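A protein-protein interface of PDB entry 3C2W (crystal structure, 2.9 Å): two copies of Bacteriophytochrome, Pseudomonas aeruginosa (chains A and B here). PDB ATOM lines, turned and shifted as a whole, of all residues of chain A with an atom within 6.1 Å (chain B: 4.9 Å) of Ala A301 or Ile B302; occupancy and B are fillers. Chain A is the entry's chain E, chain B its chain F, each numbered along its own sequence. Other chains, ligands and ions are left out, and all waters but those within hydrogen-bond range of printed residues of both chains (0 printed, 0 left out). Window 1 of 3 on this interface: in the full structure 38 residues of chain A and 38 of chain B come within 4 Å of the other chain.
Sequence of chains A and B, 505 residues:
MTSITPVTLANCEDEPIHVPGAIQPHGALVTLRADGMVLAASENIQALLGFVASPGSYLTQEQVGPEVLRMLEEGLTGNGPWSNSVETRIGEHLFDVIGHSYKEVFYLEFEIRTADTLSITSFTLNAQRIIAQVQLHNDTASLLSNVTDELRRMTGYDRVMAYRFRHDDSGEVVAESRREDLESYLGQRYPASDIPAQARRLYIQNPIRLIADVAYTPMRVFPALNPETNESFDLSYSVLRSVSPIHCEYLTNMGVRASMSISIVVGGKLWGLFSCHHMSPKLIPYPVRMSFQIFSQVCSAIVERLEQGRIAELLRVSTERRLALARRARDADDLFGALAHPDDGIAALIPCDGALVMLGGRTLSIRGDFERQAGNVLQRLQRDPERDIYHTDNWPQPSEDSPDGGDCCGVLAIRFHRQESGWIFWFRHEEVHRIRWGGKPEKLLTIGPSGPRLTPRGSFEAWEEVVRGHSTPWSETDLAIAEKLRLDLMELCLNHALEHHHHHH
Printed residues of chain B that touch a printed residue of chain A: Val B134, Gln B135, Val B298, Ile B302, Arg B305 and Leu B306.
Of the 12 printed residues of chain A, 8 touch a printed residue of chain B.
Hydrophobic or aromatic side chains of chain A within 4 Å of the printed part of chain B: Val A298, Ala A301, Ile A302 and Leu A306.
Of the printed residues of chain B, Gln A297 touches Gln B135 (2.9 Å).
Ala A301 touches just these residues of chain B: Gln B135 and Ile B302.
Printed residues of chain B within 4 Å of Ile A302: Ile B302 (3.3 Å) and Arg B305 (3.5 Å).
Val A303 touches none of the printed residues of chain B.
Printed residues of chain B within 4 Å of Arg A305: Val B134 (3.5 Å), Ile B302 (3.99 Å), Arg B305 (3.7 Å) and Leu B306 (3.5 Å).
Ser B300 touches none of the printed residues of chain A.
Of the printed residues of chain A, Ile B302 touches Ala A301, Ile A302 and Arg A305.
Of the printed residues of chain A, Arg B305 touches Ile A302, Arg A305 and Leu A306.
The nearest printed residue of chain A that does not touch Ile B302 is Val A298 (5.4 Å).
The backbone carbonyl oxygen (O) of Ser A296 sits at hydrogen-bond distance from the side-chain hydroxyl (OG) of Ser A300 (3.0 Å).
The side-chain carboxylate (OE2) of Glu A304 lies within salt-bridge range of the guanidinium group (NH1) of Arg A305, at 3.8 Å.
Ala A301 touches Ile B302, but with the chains exchanged Ile A302 does not touch Ala B301 (4.6 Å).
Ile B302 touches its own counterpart, Ile A302.
Ile A302 touches Arg B305, and with the chains exchanged Arg A305 touches Ile B302.
Arg A305 touches Leu B306, and with the chains exchanged Leu A306 touches Arg B305.
Of the 13 pairs that touch across the chains among the printed residues, 7 have their exchanged pair printed and touching as well.
CG2 of Val B298 touches CG2 of Val A298, 3.8 Å away.
CB of Ser A300 touches NE2 of Gln B135, at 3.2 Å.
Gln B135 touches Ala A301.
Ile B302 touches Ala A301 (CD1 to O, 3.2 Å).
Ile B302 touches Ile A302 (CD1 to CD1, 3.3 Å).
Arg B305 touches Ile A302 (NH1 to CG2, 3.5 Å).
Arg A305 touches Ile B302 (CD to CG1, 3.99 Å).
Arg A305 touches Arg B305 (CG to CB, 3.7 Å).
CD1 of Leu B306 touches NE of Arg A305, 3.5 Å away.
CD1 of Leu A306 touches NH2 of Arg B305 (2.9 Å).
O of Gln B135 sits close to OE2 of Glu A304.
O of Val B134 is in hydrogen-bond range of NH1 of Arg A305, 3.5 Å away.
NE2 of Gln B135 is in hydrogen-bond range of O of Gln A297 (2.9 Å).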
ATOM      1  N   ILE A 264      -6.103  -2.462 -33.517  1.00  0.00           N
ATOM      2  CA  ILE A 264      -6.076  -2.378 -32.063  1.00  0.00           C
ATOM      3  C   ILE A 264      -7.423  -2.828 -31.522  1.00  0.00           C
ATOM      4  O   ILE A 264      -8.440  -2.176 -31.746  1.00  0.00           O
ATOM      5  CB  ILE A 264      -5.777  -0.955 -31.560  1.00  0.00           C
ATOM      6  CG1 ILE A 264      -4.409  -0.483 -32.053  1.00  0.00           C
ATOM      7  CG2 ILE A 264      -5.845  -0.894 -30.040  1.00  0.00           C
ATOM      8  CD1 ILE A 264      -4.033   0.886 -31.548  1.00  0.00           C
ATOM      9  N   SER A 296       0.542  -4.894 -33.123  1.00  0.00           N
ATOM     10  CA  SER A 296      -0.913  -4.857 -32.998  1.00  0.00           C
ATOM     11  C   SER A 296      -1.365  -5.109 -31.571  1.00  0.00           C
ATOM     12  O   SER A 296      -2.129  -4.325 -31.002  1.00  0.00           O
ATOM     13  CB  SER A 296      -1.552  -5.901 -33.917  1.00  0.00           C
ATOM     14  OG  SER A 296      -2.933  -6.051 -33.654  1.00  0.00           O
ATOM     15  N   GLN A 297      -0.897  -6.214 -31.003  1.00  0.00           N
ATOM     16  CA  GLN A 297      -1.307  -6.622 -29.667  1.00  0.00           C
ATOM     17  C   GLN A 297      -0.660  -5.762 -28.588  1.00  0.00           C
ATOM     18  O   GLN A 297      -1.284  -5.457 -27.572  1.00  0.00           O
ATOM     19  CB  GLN A 297      -0.962  -8.090 -29.444  1.00  0.00           C
ATOM     20  CG  GLN A 297      -1.457  -9.029 -30.527  1.00  0.00           C
ATOM     21  CD  GLN A 297      -1.327 -10.481 -30.113  1.00  0.00           C
ATOM     22  OE1 GLN A 297      -1.415 -10.808 -28.927  1.00  0.00           O
ATOM     23  NE2 GLN A 297      -1.129 -11.360 -31.085  1.00  0.00           N
ATOM     24  N   VAL A 298       0.591  -5.375 -28.817  1.00  0.00           N
ATOM     25  CA  VAL A 298       1.309  -4.516 -27.884  1.00  0.00           C
ATOM     26  C   VAL A 298       0.496  -3.253 -27.595  1.00  0.00           C
ATOM     27  O   VAL A 298       0.146  -2.973 -26.447  1.00  0.00           O
ATOM     28  CB  VAL A 298       2.699  -4.132 -28.424  1.00  0.00           C
ATOM     29  CG1 VAL A 298       3.358  -3.094 -27.525  1.00  0.00           C
ATOM     30  CG2 VAL A 298       3.574  -5.368 -28.547  1.00  0.00           C
ATOM     31  N   CYS A 299       0.191  -2.497 -28.645  1.00  0.00           N
ATOM     32  CA  CYS A 299      -0.558  -1.258 -28.500  1.00  0.00           C
ATOM     33  C   CYS A 299      -1.940  -1.496 -27.890  1.00  0.00           C
ATOM     34  O   CYS A 299      -2.434  -0.670 -27.126  1.00  0.00           O
ATOM     35  CB  CYS A 299      -0.672  -0.538 -29.846  1.00  0.00           C
ATOM     36  SG  CYS A 299       0.905  -0.027 -30.532  1.00  0.00           S
ATOM     37  N   SER A 300      -2.558  -2.626 -28.208  1.00  0.00           N
ATOM     38  CA  SER A 300      -3.853  -2.953 -27.619  1.00  0.00           C
ATOM     39  C   SER A 300      -3.700  -3.283 -26.142  1.00  0.00           C
ATOM     40  O   SER A 300      -4.687  -3.436 -25.426  1.00  0.00           O
ATOM     41  CB  SER A 300      -4.496  -4.131 -28.352  1.00  0.00           C
ATOM     42  OG  SER A 300      -4.794  -3.794 -29.695  1.00  0.00           O
ATOM     43  N   ALA A 301      -2.451  -3.382 -25.694  1.00  0.00           N
ATOM     44  CA  ALA A 301      -2.145  -3.792 -24.325  1.00  0.00           C
ATOM     45  C   ALA A 301      -1.547  -2.672 -23.467  1.00  0.00           C
ATOM     46  O   ALA A 301      -1.519  -2.773 -22.239  1.00  0.00           O
ATOM     47  CB  ALA A 301      -1.216  -4.994 -24.333  1.00  0.00           C
ATOM     48  N   ILE A 302      -1.052  -1.619 -24.114  1.00  0.00           N
ATOM     49  CA  ILE A 302      -0.621  -0.417 -23.406  1.00  0.00           C
ATOM     50  C   ILE A 302      -1.810   0.523 -23.367  1.00  0.00           C
ATOM     51  O   ILE A 302      -2.150   1.085 -22.323  1.00  0.00           O
ATOM     52  CB  ILE A 302       0.541   0.311 -24.113  1.00  0.00           C
ATOM     53  CG1 ILE A 302       1.893  -0.326 -23.775  1.00  0.00           C
ATOM     54  CG2 ILE A 302       0.583   1.761 -23.665  1.00  0.00           C
ATOM     55  CD1 ILE A 302       1.878  -1.816 -23.704  1.00  0.00           C
ATOM     56  N   VAL A 303      -2.426   0.696 -24.530  1.00  0.00           N
ATOM     57  CA  VAL A 303      -3.657   1.453 -24.650  1.00  0.00           C
ATOM     58  C   VAL A 303      -4.739   0.841 -23.763  1.00  0.00           C
ATOM     59  O   VAL A 303      -5.664   1.529 -23.333  1.00  0.00           O
ATOM     60  CB  VAL A 303      -4.124   1.498 -26.120  1.00  0.00           C
ATOM     61  CG1 VAL A 303      -5.605   1.864 -26.218  1.00  0.00           C
ATOM     62  CG2 VAL A 303      -3.254   2.467 -26.912  1.00  0.00           C
ATOM     63  N   GLU A 304      -4.613  -0.451 -23.476  1.00  0.00           N
ATOM     64  CA  GLU A 304      -5.538  -1.115 -22.564  1.00  0.00           C
ATOM     65  C   GLU A 304      -5.581  -0.375 -21.233  1.00  0.00           C
ATOM     66  O   GLU A 304      -6.644   0.084 -20.801  1.00  0.00           O
ATOM     67  CB  GLU A 304      -5.142  -2.581 -22.339  1.00  0.00           C
ATOM     68  CG  GLU A 304      -5.770  -3.238 -21.097  1.00  0.00           C
ATOM     69  CD  GLU A 304      -7.077  -3.959 -21.386  1.00  0.00           C
ATOM     70  OE1 GLU A 304      -8.080  -3.284 -21.708  1.00  0.00           O
ATOM     71  OE2 GLU A 304      -7.111  -5.202 -21.258  1.00  0.00           O
ATOM     72  N   ARG A 305      -4.418  -0.251 -20.593  1.00  0.00           N
ATOM     73  CA  ARG A 305      -4.337   0.358 -19.265  1.00  0.00           C
ATOM     74  C   ARG A 305      -3.967   1.847 -19.251  1.00  0.00           C
ATOM     75  O   ARG A 305      -3.833   2.438 -18.179  1.00  0.00           O
ATOM     76  CB  ARG A 305      -3.424  -0.441 -18.315  1.00  0.00           C
ATOM     77  CG  ARG A 305      -2.293  -1.207 -18.971  1.00  0.00           C
ATOM     78  CD  ARG A 305      -2.752  -2.586 -19.445  1.00  0.00           C
ATOM     79  NE  ARG A 305      -3.687  -3.203 -18.505  1.00  0.00           N
ATOM     80  CZ  ARG A 305      -4.132  -4.453 -18.604  1.00  0.00           C
ATOM     81  NH1 ARG A 305      -3.731  -5.224 -19.605  1.00  0.00           N
ATOM     82  NH2 ARG A 305      -4.982  -4.932 -17.708  1.00  0.00           N
ATOM     83  N   LEU A 306      -3.812   2.454 -20.424  1.00  0.00           N
ATOM     84  CA  LEU A 306      -3.695   3.908 -20.478  1.00  0.00           C
ATOM     85  C   LEU A 306      -5.055   4.543 -20.253  1.00  0.00           C
ATOM     86  O   LEU A 306      -5.201   5.443 -19.430  1.00  0.00           O
ATOM     87  CB  LEU A 306      -3.099   4.385 -21.798  1.00  0.00           C
ATOM     88  CG  LEU A 306      -1.643   4.805 -21.662  1.00  0.00           C
ATOM     89  CD1 LEU A 306      -0.903   3.707 -20.939  1.00  0.00           C
ATOM     90  CD2 LEU A 306      -1.014   5.109 -23.004  1.00  0.00           C
ATOM     91  N   VAL B 134      -0.615 -11.229 -21.306  1.00  0.00           N
ATOM     92  CA  VAL B 134      -0.438  -9.983 -20.574  1.00  0.00           C
ATOM     93  C   VAL B 134      -1.654  -9.086 -20.813  1.00  0.00           C
ATOM     94  O   VAL B 134      -1.972  -8.224 -19.999  1.00  0.00           O
ATOM     95  CB  VAL B 134       0.873  -9.278 -21.000  1.00  0.00           C
ATOM     96  CG1 VAL B 134       0.591  -8.148 -21.985  1.00  0.00           C
ATOM     97  CG2 VAL B 134       1.633  -8.760 -19.785  1.00  0.00           C
ATOM     98  N   GLN B 135      -2.336  -9.324 -21.929  1.00  0.00           N
ATOM     99  CA  GLN B 135      -3.520  -8.565 -22.323  1.00  0.00           C
ATOM    100  C   GLN B 135      -4.802  -8.974 -21.611  1.00  0.00           C
ATOM    101  O   GLN B 135      -5.847  -8.378 -21.847  1.00  0.00           O
ATOM    102  CB  GLN B 135      -3.785  -8.759 -23.814  1.00  0.00           C
ATOM    103  CG  GLN B 135      -3.014  -7.896 -24.776  1.00  0.00           C
ATOM    104  CD  GLN B 135      -3.572  -8.006 -26.179  1.00  0.00           C
ATOM    105  OE1 GLN B 135      -3.924  -9.096 -26.628  1.00  0.00           O
ATOM    106  NE2 GLN B 135      -3.667  -6.881 -26.873  1.00  0.00           N
ATOM    107  N   LEU B 143      -1.405 -11.579 -13.478  1.00  0.00           N
ATOM    108  CA  LEU B 143      -0.418 -11.514 -14.544  1.00  0.00           C
ATOM    109  C   LEU B 143       0.829 -12.331 -14.202  1.00  0.00           C
ATOM    110  O   LEU B 143       1.462 -12.898 -15.084  1.00  0.00           O
ATOM    111  CB  LEU B 143      -0.021 -10.069 -14.845  1.00  0.00           C
ATOM    112  CG  LEU B 143       1.087  -9.979 -15.900  1.00  0.00           C
ATOM    113  CD1 LEU B 143       0.589 -10.564 -17.203  1.00  0.00           C
ATOM    114  CD2 LEU B 143       1.553  -8.557 -16.099  1.00  0.00           C
ATOM    115  N   VAL B 298       7.694  -5.780 -22.947  1.00  0.00           N
ATOM    116  CA  VAL B 298       6.273  -5.452 -22.866  1.00  0.00           C
ATOM    117  C   VAL B 298       5.707  -5.747 -21.482  1.00  0.00           C
ATOM    118  O   VAL B 298       4.904  -4.979 -20.956  1.00  0.00           O
ATOM    119  CB  VAL B 298       5.450  -6.213 -23.919  1.00  0.00           C
ATOM    120  CG1 VAL B 298       4.105  -6.654 -23.334  1.00  0.00           C
ATOM    121  CG2 VAL B 298       5.259  -5.358 -25.160  1.00  0.00           C
ATOM    122  N   CYS B 299       6.135  -6.860 -20.896  1.00  0.00           N
ATOM    123  CA  CYS B 299       5.669  -7.253 -19.571  1.00  0.00           C
ATOM    124  C   CYS B 299       6.121  -6.266 -18.496  1.00  0.00           C
ATOM    125  O   CYS B 299       5.346  -5.916 -17.604  1.00  0.00           O
ATOM    126  CB  CYS B 299       6.120  -8.670 -19.224  1.00  0.00           C
ATOM    127  SG  CYS B 299       5.310  -9.363 -17.778  1.00  0.00           S
ATOM    128  N   SER B 300       7.369  -5.815 -18.576  1.00  0.00           N
ATOM    129  CA  SER B 300       7.831  -4.743 -17.701  1.00  0.00           C
ATOM    130  C   SER B 300       6.982  -3.502 -17.915  1.00  0.00           C
ATOM    131  O   SER B 300       6.716  -2.751 -16.984  1.00  0.00           O
ATOM    132  CB  SER B 300       9.298  -4.417 -17.976  1.00  0.00           C
ATOM    133  OG  SER B 300      10.155  -5.361 -17.357  1.00  0.00           O
ATOM    134  N   ALA B 301       6.560  -3.296 -19.156  1.00  0.00           N
ATOM    135  CA  ALA B 301       5.715  -2.162 -19.512  1.00  0.00           C
ATOM    136  C   ALA B 301       4.316  -2.278 -18.904  1.00  0.00           C
ATOM    137  O   ALA B 301       3.749  -1.282 -18.465  1.00  0.00           O
ATOM    138  CB  ALA B 301       5.629  -2.014 -21.028  1.00  0.00           C
ATOM    139  N   ILE B 302       3.767  -3.491 -18.881  1.00  0.00           N
ATOM    140  CA  ILE B 302       2.431  -3.725 -18.330  1.00  0.00           C
ATOM    141  C   ILE B 302       2.431  -3.864 -16.804  1.00  0.00           C
ATOM    142  O   ILE B 302       1.435  -3.556 -16.148  1.00  0.00           O
ATOM    143  CB  ILE B 302       1.739  -4.939 -18.984  1.00  0.00           C
ATOM    144  CG1 ILE B 302       0.716  -4.477 -20.029  1.00  0.00           C
ATOM    145  CG2 ILE B 302       1.032  -5.771 -17.944  1.00  0.00           C
ATOM    146  CD1 ILE B 302       1.329  -3.970 -21.299  1.00  0.00           C
ATOM    147  N   VAL B 303       3.540  -4.332 -16.241  1.00  0.00           N
ATOM    148  CA  VAL B 303       3.694  -4.344 -14.790  1.00  0.00           C
ATOM    149  C   VAL B 303       3.853  -2.902 -14.334  1.00  0.00           C
ATOM    150  O   VAL B 303       3.424  -2.523 -13.243  1.00  0.00           O
ATOM    151  CB  VAL B 303       4.926  -5.155 -14.341  1.00  0.00           C
ATOM    152  CG1 VAL B 303       5.177  -4.972 -12.852  1.00  0.00           C
ATOM    153  CG2 VAL B 303       4.740  -6.626 -14.675  1.00  0.00           C
ATOM    154  N   GLU B 304       4.481  -2.106 -15.191  1.00  0.00           N
ATOM    155  CA  GLU B 304       4.627  -0.678 -14.974  1.00  0.00           C
ATOM    156  C   GLU B 304       3.269  -0.032 -14.703  1.00  0.00           C
ATOM    157  O   GLU B 304       3.089   0.622 -13.679  1.00  0.00           O
ATOM    158  CB  GLU B 304       5.283  -0.041 -16.201  1.00  0.00           C
ATOM    159  CG  GLU B 304       5.141   1.468 -16.286  1.00  0.00           C
ATOM    160  CD  GLU B 304       6.207   2.207 -15.508  1.00  0.00           C
ATOM    161  OE1 GLU B 304       7.001   1.534 -14.815  1.00  0.00           O
ATOM    162  OE2 GLU B 304       6.242   3.454 -15.594  1.00  0.00           O
ATOM    163  N   ARG B 305       2.315  -0.227 -15.612  1.00  0.00           N
ATOM    164  CA  ARG B 305       0.995   0.391 -15.478  1.00  0.00           C
ATOM    165  C   ARG B 305       0.152  -0.284 -14.397  1.00  0.00           C
ATOM    166  O   ARG B 305      -0.642   0.367 -13.719  1.00  0.00           O
ATOM    167  CB  ARG B 305       0.220   0.375 -16.799  1.00  0.00           C
ATOM    168  CG  ARG B 305       1.054   0.320 -18.066  1.00  0.00           C
ATOM    169  CD  ARG B 305       2.230   1.282 -18.038  1.00  0.00           C
ATOM    170  NE  ARG B 305       1.920   2.627 -18.514  1.00  0.00           N
ATOM    171  CZ  ARG B 305       2.057   3.024 -19.776  1.00  0.00           C
ATOM    172  NH1 ARG B 305       2.480   2.171 -20.695  1.00  0.00           N
ATOM    173  NH2 ARG B 305       1.774   4.276 -20.114  1.00  0.00           N
ATOM    174  N   LEU B 306       0.305  -1.593 -14.245  1.00  0.00           N
ATOM    175  CA  LEU B 306      -0.476  -2.322 -13.248  1.00  0.00           C
ATOM    176  C   LEU B 306      -0.068  -1.979 -11.817  1.00  0.00           C
ATOM    177  O   LEU B 306      -0.779  -2.304 -10.866  1.00  0.00           O
ATOM    178  CB  LEU B 306      -0.411  -3.837 -13.482  1.00  0.00           C
ATOM    179  CG  LEU B 306      -1.573  -4.399 -14.308  1.00  0.00           C
ATOM    180  CD1 LEU B 306      -1.583  -3.798 -15.709  1.00  0.00           C
ATOM    181  CD2 LEU B 306      -1.511  -5.912 -14.358  1.00  0.00           C
